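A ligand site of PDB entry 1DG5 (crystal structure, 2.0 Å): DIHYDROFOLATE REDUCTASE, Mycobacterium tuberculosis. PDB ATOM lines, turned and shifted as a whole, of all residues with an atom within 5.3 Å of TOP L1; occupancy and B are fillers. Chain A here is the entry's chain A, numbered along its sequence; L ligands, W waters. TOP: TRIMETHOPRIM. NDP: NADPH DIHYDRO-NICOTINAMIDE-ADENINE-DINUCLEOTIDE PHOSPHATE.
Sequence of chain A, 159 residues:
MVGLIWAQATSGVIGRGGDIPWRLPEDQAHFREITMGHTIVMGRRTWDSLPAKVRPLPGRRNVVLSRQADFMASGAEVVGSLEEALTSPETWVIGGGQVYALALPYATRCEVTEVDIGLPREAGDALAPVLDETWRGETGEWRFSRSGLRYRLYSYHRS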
ATOM      1  N   ILE A   5     -23.082  22.390  -7.573  1.00  0.00           N
ATOM      2  CA  ILE A   5     -21.889  22.478  -6.737  1.00  0.00           C
ATOM      3  C   ILE A   5     -20.745  23.042  -7.561  1.00  0.00           C
ATOM      4  O   ILE A   5     -20.527  22.636  -8.708  1.00  0.00           O
ATOM      5  CB  ILE A   5     -21.520  21.116  -6.057  1.00  0.00           C
ATOM      6  CG1 ILE A   5     -20.238  21.268  -5.233  1.00  0.00           C
ATOM      7  CG2 ILE A   5     -21.362  20.007  -7.081  1.00  0.00           C
ATOM      8  CD1 ILE A   5     -19.968  20.096  -4.293  1.00  0.00           C
ATOM      9  N   TRP A   6     -20.066  24.043  -7.012  1.00  0.00           N
ATOM     10  CA  TRP A   6     -18.934  24.664  -7.686  1.00  0.00           C
ATOM     11  C   TRP A   6     -18.036  25.409  -6.705  1.00  0.00           C
ATOM     12  O   TRP A   6     -18.421  25.658  -5.555  1.00  0.00           O
ATOM     13  CB  TRP A   6     -19.414  25.661  -8.757  1.00  0.00           C
ATOM     14  CG  TRP A   6     -20.008  26.974  -8.234  1.00  0.00           C
ATOM     15  CD1 TRP A   6     -19.326  28.104  -7.879  1.00  0.00           C
ATOM     16  CD2 TRP A   6     -21.399  27.269  -8.034  1.00  0.00           C
ATOM     17  NE1 TRP A   6     -20.197  29.091  -7.482  1.00  0.00           N
ATOM     18  CE2 TRP A   6     -21.472  28.603  -7.558  1.00  0.00           C
ATOM     19  CE3 TRP A   6     -22.585  26.537  -8.206  1.00  0.00           C
ATOM     20  CZ2 TRP A   6     -22.694  29.221  -7.263  1.00  0.00           C
ATOM     21  CZ3 TRP A   6     -23.793  27.153  -7.915  1.00  0.00           C
ATOM     22  CH2 TRP A   6     -23.839  28.483  -7.447  1.00  0.00           C
ATOM     23  N   ALA A   7     -16.856  25.767  -7.173  1.00  0.00           N
ATOM     24  CA  ALA A   7     -15.872  26.530  -6.424  1.00  0.00           C
ATOM     25  C   ALA A   7     -15.614  27.784  -7.275  1.00  0.00           C
ATOM     26  O   ALA A   7     -15.334  27.684  -8.469  1.00  0.00           O
ATOM     27  CB  ALA A   7     -14.573  25.713  -6.261  1.00  0.00           C
ATOM     28  N   ILE A  20      -9.336  25.166 -13.893  1.00  0.00           N
ATOM     29  CA  ILE A  20      -9.795  25.853 -12.694  1.00  0.00           C
ATOM     30  C   ILE A  20      -8.534  26.675 -12.420  1.00  0.00           C
ATOM     31  O   ILE A  20      -7.453  26.118 -12.269  1.00  0.00           O
ATOM     32  CB  ILE A  20     -10.093  24.877 -11.558  1.00  0.00           C
ATOM     33  CG1 ILE A  20     -11.366  24.089 -11.860  1.00  0.00           C
ATOM     34  CG2 ILE A  20     -10.248  25.639 -10.264  1.00  0.00           C
ATOM     35  CD1 ILE A  20     -11.873  23.219 -10.726  1.00  0.00           C
ATOM     36  N   ASP A  27     -10.548  20.938  -1.685  1.00  0.00           N
ATOM     37  CA  ASP A  27     -11.778  21.010  -2.453  1.00  0.00           C
ATOM     38  C   ASP A  27     -12.231  19.624  -2.887  1.00  0.00           C
ATOM     39  O   ASP A  27     -13.402  19.268  -2.720  1.00  0.00           O
ATOM     40  CB  ASP A  27     -11.564  21.921  -3.680  1.00  0.00           C
ATOM     41  CG  ASP A  27     -12.800  22.033  -4.558  1.00  0.00           C
ATOM     42  OD1 ASP A  27     -13.824  22.597  -4.132  1.00  0.00           O
ATOM     43  OD2 ASP A  27     -12.736  21.587  -5.723  1.00  0.00           O
ATOM     44  N   GLN A  28     -11.282  18.846  -3.373  1.00  0.00           N
ATOM     45  CA  GLN A  28     -11.546  17.495  -3.863  1.00  0.00           C
ATOM     46  C   GLN A  28     -12.348  16.629  -2.903  1.00  0.00           C
ATOM     47  O   GLN A  28     -13.275  15.925  -3.315  1.00  0.00           O
ATOM     48  CB  GLN A  28     -10.216  16.813  -4.209  1.00  0.00           C
ATOM     49  CG  GLN A  28      -9.278  17.724  -4.998  1.00  0.00           C
ATOM     50  CD  GLN A  28      -7.793  17.349  -4.865  1.00  0.00           C
ATOM     51  OE1 GLN A  28      -7.370  16.779  -3.849  1.00  0.00           O
ATOM     52  NE2 GLN A  28      -7.006  17.696  -5.880  1.00  0.00           N
ATOM     53  N   PHE A  31     -15.984  18.083  -2.397  1.00  0.00           N
ATOM     54  CA  PHE A  31     -16.750  17.767  -3.594  1.00  0.00           C
ATOM     55  C   PHE A  31     -17.165  16.299  -3.536  1.00  0.00           C
ATOM     56  O   PHE A  31     -18.320  15.954  -3.775  1.00  0.00           O
ATOM     57  CB  PHE A  31     -15.876  18.044  -4.823  1.00  0.00           C
ATOM     58  CG  PHE A  31     -16.467  17.562  -6.122  1.00  0.00           C
ATOM     59  CD1 PHE A  31     -17.536  18.224  -6.713  1.00  0.00           C
ATOM     60  CD2 PHE A  31     -15.920  16.452  -6.772  1.00  0.00           C
ATOM     61  CE1 PHE A  31     -18.062  17.787  -7.924  1.00  0.00           C
ATOM     62  CE2 PHE A  31     -16.437  16.016  -7.978  1.00  0.00           C
ATOM     63  CZ  PHE A  31     -17.514  16.693  -8.555  1.00  0.00           C
ATOM     64  N   THR A  46     -16.743  20.220 -19.405  1.00  0.00           N
ATOM     65  CA  THR A  46     -16.287  19.866 -18.058  1.00  0.00           C
ATOM     66  C   THR A  46     -15.759  18.426 -18.115  1.00  0.00           C
ATOM     67  O   THR A  46     -14.734  18.112 -17.523  1.00  0.00           O
ATOM     68  CB  THR A  46     -17.420  20.006 -17.019  1.00  0.00           C
ATOM     69  OG1 THR A  46     -17.726  21.393 -16.855  1.00  0.00           O
ATOM     70  CG2 THR A  46     -16.987  19.462 -15.679  1.00  0.00           C
ATOM     71  N   SER A  49     -12.444  18.464 -19.449  1.00  0.00           N
ATOM     72  CA  SER A  49     -11.576  19.069 -18.449  1.00  0.00           C
ATOM     73  C   SER A  49     -11.110  18.059 -17.392  1.00  0.00           C
ATOM     74  O   SER A  49     -10.068  18.236 -16.768  1.00  0.00           O
ATOM     75  CB  SER A  49     -12.332  20.221 -17.767  1.00  0.00           C
ATOM     76  OG  SER A  49     -11.498  20.940 -16.881  1.00  0.00           O
ATOM     77  N   LEU A  50     -11.884  17.005 -17.176  1.00  0.00           N
ATOM     78  CA  LEU A  50     -11.493  15.997 -16.194  1.00  0.00           C
ATOM     79  C   LEU A  50     -10.266  15.222 -16.656  1.00  0.00           C
ATOM     80  O   LEU A  50     -10.167  14.824 -17.831  1.00  0.00           O
ATOM     81  CB  LEU A  50     -12.639  15.012 -15.955  1.00  0.00           C
ATOM     82  CG  LEU A  50     -13.936  15.499 -15.315  1.00  0.00           C
ATOM     83  CD1 LEU A  50     -14.942  14.363 -15.271  1.00  0.00           C
ATOM     84  CD2 LEU A  50     -13.662  16.008 -13.917  1.00  0.00           C
ATOM     85  N   PRO A  51      -9.265  15.045 -15.759  1.00  0.00           N
ATOM     86  CA  PRO A  51      -8.073  14.293 -16.153  1.00  0.00           C
ATOM     87  C   PRO A  51      -8.520  12.876 -16.550  1.00  0.00           C
ATOM     88  O   PRO A  51      -9.412  12.301 -15.921  1.00  0.00           O
ATOM     89  CB  PRO A  51      -7.264  14.258 -14.862  1.00  0.00           C
ATOM     90  CG  PRO A  51      -7.635  15.542 -14.193  1.00  0.00           C
ATOM     91  CD  PRO A  51      -9.133  15.583 -14.396  1.00  0.00           C
ATOM     92  N   VAL A  54      -8.918  10.186 -13.919  1.00  0.00           N
ATOM     93  CA  VAL A  54      -9.980  10.314 -12.909  1.00  0.00           C
ATOM     94  C   VAL A  54     -11.404  10.215 -13.449  1.00  0.00           C
ATOM     95  O   VAL A  54     -12.347  10.195 -12.658  1.00  0.00           O
ATOM     96  CB  VAL A  54      -9.836  11.619 -12.044  1.00  0.00           C
ATOM     97  CG1 VAL A  54      -8.371  11.898 -11.695  1.00  0.00           C
ATOM     98  CG2 VAL A  54     -10.464  12.825 -12.732  1.00  0.00           C
ATOM     99  N   LEU A  57     -15.852   9.896 -12.856  1.00  0.00           N
ATOM    100  CA  LEU A  57     -15.661  10.024 -11.419  1.00  0.00           C
ATOM    101  C   LEU A  57     -16.223   8.767 -10.769  1.00  0.00           C
ATOM    102  O   LEU A  57     -17.400   8.429 -10.986  1.00  0.00           O
ATOM    103  CB  LEU A  57     -16.366  11.258 -10.904  1.00  0.00           C
ATOM    104  CG  LEU A  57     -15.786  12.536 -11.481  1.00  0.00           C
ATOM    105  CD1 LEU A  57     -16.524  13.739 -10.937  1.00  0.00           C
ATOM    106  CD2 LEU A  57     -14.310  12.590 -11.111  1.00  0.00           C
ATOM    107  N   VAL A  93     -25.283  18.805 -10.257  1.00  0.00           N
ATOM    108  CA  VAL A  93     -24.745  19.408 -11.473  1.00  0.00           C
ATOM    109  C   VAL A  93     -23.355  19.890 -11.055  1.00  0.00           C
ATOM    110  O   VAL A  93     -23.203  20.764 -10.193  1.00  0.00           O
ATOM    111  CB  VAL A  93     -25.690  20.552 -11.975  1.00  0.00           C
ATOM    112  CG1 VAL A  93     -25.051  21.297 -13.152  1.00  0.00           C
ATOM    113  CG2 VAL A  93     -27.056  19.951 -12.399  1.00  0.00           C
ATOM    114  N   ILE A  94     -22.334  19.261 -11.625  1.00  0.00           N
ATOM    115  CA  ILE A  94     -20.962  19.563 -11.249  1.00  0.00           C
ATOM    116  C   ILE A  94     -20.240  20.454 -12.211  1.00  0.00           C
ATOM    117  O   ILE A  94     -19.017  20.632 -12.128  1.00  0.00           O
ATOM    118  CB  ILE A  94     -20.135  18.288 -11.057  1.00  0.00           C
ATOM    119  CG1 ILE A  94     -19.886  17.601 -12.398  1.00  0.00           C
ATOM    120  CG2 ILE A  94     -20.864  17.359 -10.121  1.00  0.00           C
ATOM    121  CD1 ILE A  94     -18.643  16.730 -12.387  1.00  0.00           C
ATOM    122  N   GLY A  95     -20.950  21.018 -13.160  1.00  0.00           N
ATOM    123  CA  GLY A  95     -20.208  21.857 -14.012  1.00  0.00           C
ATOM    124  C   GLY A  95     -20.596  22.231 -15.389  1.00  0.00           C
ATOM    125  O   GLY A  95     -21.138  21.452 -16.177  1.00  0.00           O
ATOM    126  N   TYR A 100     -24.521  25.194 -15.547  1.00  0.00           N
ATOM    127  CA  TYR A 100     -25.043  25.726 -14.281  1.00  0.00           C
ATOM    128  C   TYR A 100     -26.195  26.679 -14.590  1.00  0.00           C
ATOM    129  O   TYR A 100     -27.199  26.704 -13.868  1.00  0.00           O
ATOM    130  CB  TYR A 100     -23.978  26.497 -13.493  1.00  0.00           C
ATOM    131  CG  TYR A 100     -22.904  25.674 -12.811  1.00  0.00           C
ATOM    132  CD1 TYR A 100     -21.563  26.039 -12.918  1.00  0.00           C
ATOM    133  CD2 TYR A 100     -23.223  24.544 -12.044  1.00  0.00           C
ATOM    134  CE1 TYR A 100     -20.557  25.305 -12.299  1.00  0.00           C
ATOM    135  CE2 TYR A 100     -22.216  23.800 -11.423  1.00  0.00           C
ATOM    136  CZ  TYR A 100     -20.887  24.189 -11.555  1.00  0.00           C
ATOM    137  OH  TYR A 100     -19.864  23.507 -10.935  1.00  0.00           O
ATOM    138  N   THR A 113     -18.096  26.919  -2.826  1.00  0.00           N
ATOM    139  CA  THR A 113     -16.819  27.136  -2.166  1.00  0.00           C
ATOM    140  C   THR A 113     -16.307  28.469  -2.680  1.00  0.00           C
ATOM    141  O   THR A 113     -16.138  28.635  -3.880  1.00  0.00           O
ATOM    142  CB  THR A 113     -15.802  26.041  -2.546  1.00  0.00           C
ATOM    143  OG1 THR A 113     -16.256  24.783  -2.052  1.00  0.00           O
ATOM    144  CG2 THR A 113     -14.420  26.365  -1.963  1.00  0.00           C
HETATM  145  C1  TOP L   1     -14.878  20.589  -8.330  1.00  0.00           C
HETATM  146  N2  TOP L   1     -14.963  21.233  -7.137  1.00  0.00           N
HETATM  147  C3  TOP L   1     -16.128  21.742  -6.777  1.00  0.00           C
HETATM  148  N4  TOP L   1     -16.228  22.369  -5.573  1.00  0.00           N
HETATM  149  N5  TOP L   1     -17.319  21.726  -7.448  1.00  0.00           N
HETATM  150  C6  TOP L   1     -17.286  21.110  -8.630  1.00  0.00           C
HETATM  151  N7  TOP L   1     -18.389  21.035  -9.378  1.00  0.00           N
HETATM  152  C8  TOP L   1     -15.992  20.490  -9.122  1.00  0.00           C
HETATM  153  C9  TOP L   1     -15.937  19.769 -10.469  1.00  0.00           C
HETATM  154  C10 TOP L   1     -14.595  19.215 -10.841  1.00  0.00           C
HETATM  155  C11 TOP L   1     -13.925  19.882 -11.859  1.00  0.00           C
HETATM  156  C12 TOP L   1     -12.644  19.455 -12.270  1.00  0.00           C
HETATM  157  O13 TOP L   1     -11.944  20.083 -13.272  1.00  0.00           O
HETATM  158  C14 TOP L   1     -12.594  21.128 -13.976  1.00  0.00           C
HETATM  159  C15 TOP L   1     -12.069  18.359 -11.610  1.00  0.00           C
HETATM  160  O16 TOP L   1     -10.784  17.914 -11.977  1.00  0.00           O
HETATM  161  C17 TOP L   1      -9.886  18.657 -11.207  1.00  0.00           C
HETATM  162  C18 TOP L   1     -12.740  17.673 -10.586  1.00  0.00           C
HETATM  163  O19 TOP L   1     -12.052  16.593 -10.025  1.00  0.00           O
HETATM  164  C20 TOP L   1     -12.626  16.213  -8.773  1.00  0.00           C
HETATM  165  C21 TOP L   1     -14.022  18.090 -10.172  1.00  0.00           C
HETATM  166  PA  NDP L   2     -19.705  23.249 -19.961  1.00  0.00           P
HETATM  167  O1A NDP L   2     -20.926  23.807 -19.353  1.00  0.00           O
HETATM  168  O2A NDP L   2     -19.005  22.315 -19.057  1.00  0.00           O
HETATM  169  O5B NDP L   2     -20.043  22.475 -21.314  1.00  0.00           O
HETATM  170  C5B NDP L   2     -20.702  23.230 -22.383  1.00  0.00           C
HETATM  171  C4B NDP L   2     -21.081  22.118 -23.375  1.00  0.00           C
HETATM  172  O4B NDP L   2     -22.238  21.452 -22.851  1.00  0.00           O
HETATM  173  C3B NDP L   2     -21.520  22.626 -24.765  1.00  0.00           C
HETATM  174  O3B NDP L   2     -20.364  22.945 -25.500  1.00  0.00           O
HETATM  175  C2B NDP L   2     -22.330  21.364 -25.199  1.00  0.00           C
HETATM  176  O2B NDP L   2     -21.569  20.256 -25.600  1.00  0.00           O
HETATM  177  C1B NDP L   2     -23.083  21.089 -23.945  1.00  0.00           C
HETATM  178  N9A NDP L   2     -24.308  21.813 -23.851  1.00  0.00           N
HETATM  179  C8A NDP L   2     -24.514  23.075 -23.360  1.00  0.00           C
HETATM  180  N7A NDP L   2     -25.785  23.423 -23.374  1.00  0.00           N
HETATM  181  C5A NDP L   2     -26.425  22.333 -23.897  1.00  0.00           C
HETATM  182  C6A NDP L   2     -27.807  22.104 -24.173  1.00  0.00           C
HETATM  183  N6A NDP L   2     -28.706  23.055 -23.896  1.00  0.00           N
HETATM  184  N1A NDP L   2     -28.139  20.899 -24.711  1.00  0.00           N
HETATM  185  C2A NDP L   2     -27.134  19.992 -24.961  1.00  0.00           C
HETATM  186  N3A NDP L   2     -25.856  20.122 -24.752  1.00  0.00           N
HETATM  187  C4A NDP L   2     -25.564  21.324 -24.198  1.00  0.00           C
HETATM  188  O3  NDP L   2     -18.752  24.365 -20.423  1.00  0.00           O
HETATM  189  PN  NDP L   2     -18.159  25.763 -20.028  1.00  0.00           P
HETATM  190  O1N NDP L   2     -17.216  26.248 -21.045  1.00  0.00           O
HETATM  191  O2N NDP L   2     -19.245  26.723 -19.755  1.00  0.00           O
HETATM  192  O5D NDP L   2     -17.403  25.480 -18.599  1.00  0.00           O
HETATM  193  C5D NDP L   2     -16.153  24.736 -18.650  1.00  0.00           C
HETATM  194  C4D NDP L   2     -15.203  25.470 -17.662  1.00  0.00           C
HETATM  195  O4D NDP L   2     -15.732  25.371 -16.306  1.00  0.00           O
HETATM  196  C3D NDP L   2     -13.795  24.839 -17.624  1.00  0.00           C
HETATM  197  O3D NDP L   2     -12.833  25.895 -17.629  1.00  0.00           O
HETATM  198  C2D NDP L   2     -13.860  24.032 -16.309  1.00  0.00           C
HETATM  199  O2D NDP L   2     -12.540  23.787 -15.812  1.00  0.00           O
HETATM  200  C1D NDP L   2     -14.683  24.938 -15.415  1.00  0.00           C
HETATM  201  N1N NDP L   2     -15.285  24.199 -14.245  1.00  0.00           N
HETATM  202  C2N NDP L   2     -15.104  24.810 -12.975  1.00  0.00           C
HETATM  203  C3N NDP L   2     -15.657  24.151 -11.877  1.00  0.00           C
HETATM  204  C7N NDP L   2     -15.469  24.824 -10.472  1.00  0.00           C
HETATM  205  O7N NDP L   2     -16.104  24.388  -9.548  1.00  0.00           O
HETATM  206  N7N NDP L   2     -14.593  25.864 -10.410  1.00  0.00           N
HETATM  207  C4N NDP L   2     -16.395  22.917 -11.933  1.00  0.00           C
HETATM  208  C5N NDP L   2     -16.490  22.411 -13.288  1.00  0.00           C
HETATM  209  C6N NDP L   2     -15.977  22.994 -14.404  1.00  0.00           C
HETATM  210  P2B NDP L   2     -21.228  20.101 -27.236  1.00  0.00           P
HETATM  211  O1X NDP L   2     -20.504  21.299 -27.609  1.00  0.00           O
HETATM  212  O2X NDP L   2     -20.437  18.830 -27.110  1.00  0.00           O
HETATM  213  O3X NDP L   2     -22.581  19.980 -27.803  1.00  0.00           O
HETATM  214  O   HOH W   1     -18.308  23.455  -3.296  1.00  0.00           O
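A nitrogen (N2) of TOP L1 sits at hydrogen-bond distance from the side-chain carboxylate (OD2) of Asp 27 (2.7 Å).
A nitrogen (N7) of TOP L1 lies within hydrogen-bond range of the backbone carbonyl oxygen (O) of Ile 5 (2.8 Å).
N7 of TOP L1 is in hydrogen-bond range of O of Ile 94 (2.8 Å).
OH of Tyr 100 is in hydrogen-bond range of N7 of TOP L1, 3.3 Å away.
The side-chain hydroxyl (OG) of Ser 49 lies within hydrogen-bond range of an oxygen (O2D) of NDP L2, at 3.2 Å.
The backbone NH of Ala 7 lies within hydrogen-bond range of an oxygen (O7N) of NDP L2 (2.8 Å).
A nitrogen (N7N) of NDP L2 lies within hydrogen-bond range of the backbone carbonyl oxygen of Ala 7 (2.8 Å).
The backbone NH (N) of Thr 46 is in hydrogen-bond range of an oxygen (O2A) of NDP L2, 3.1 Å away.
The side-chain hydroxyl of Thr 46 sits at hydrogen-bond distance from an oxygen (O2A) of NDP L2 (2.7 Å).
OH of Tyr 100 lies within hydrogen-bond range of O of Ile 5, at 2.5 Å.
N of Ile 5 lies within hydrogen-bond range of O of Val 93 (3.1 Å).
The backbone carbonyl oxygen of Ile 94 is in hydrogen-bond range of the side-chain hydroxyl of Tyr 100 (3.2 Å).
The backbone carbonyl oxygen of Trp 6 is in hydrogen-bond range of the backbone NH of Thr 113.
CA of Trp 6 touches N5 of TOP L1 (3.4 Å).
CB of Ala 7 touches N4 of TOP L1 (3.8 Å).
Ile 20 touches TOP L1 (CG1 to C14, 3.8 Å).
CD1 of Phe 31 touches C6 of TOP L1, 3.5 Å away.
Ser 49 touches TOP L1 (OG to C14, 3.1 Å).
Leu 50 touches TOP L1 (CD2 to C15, 3.7 Å).
CD of Pro 51 touches O16 of TOP L1, 3.7 Å away.
Water W1 lies within hydrogen-bond range of OG1 of Thr 113, O of Trp 6 and N4 of TOP L1.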
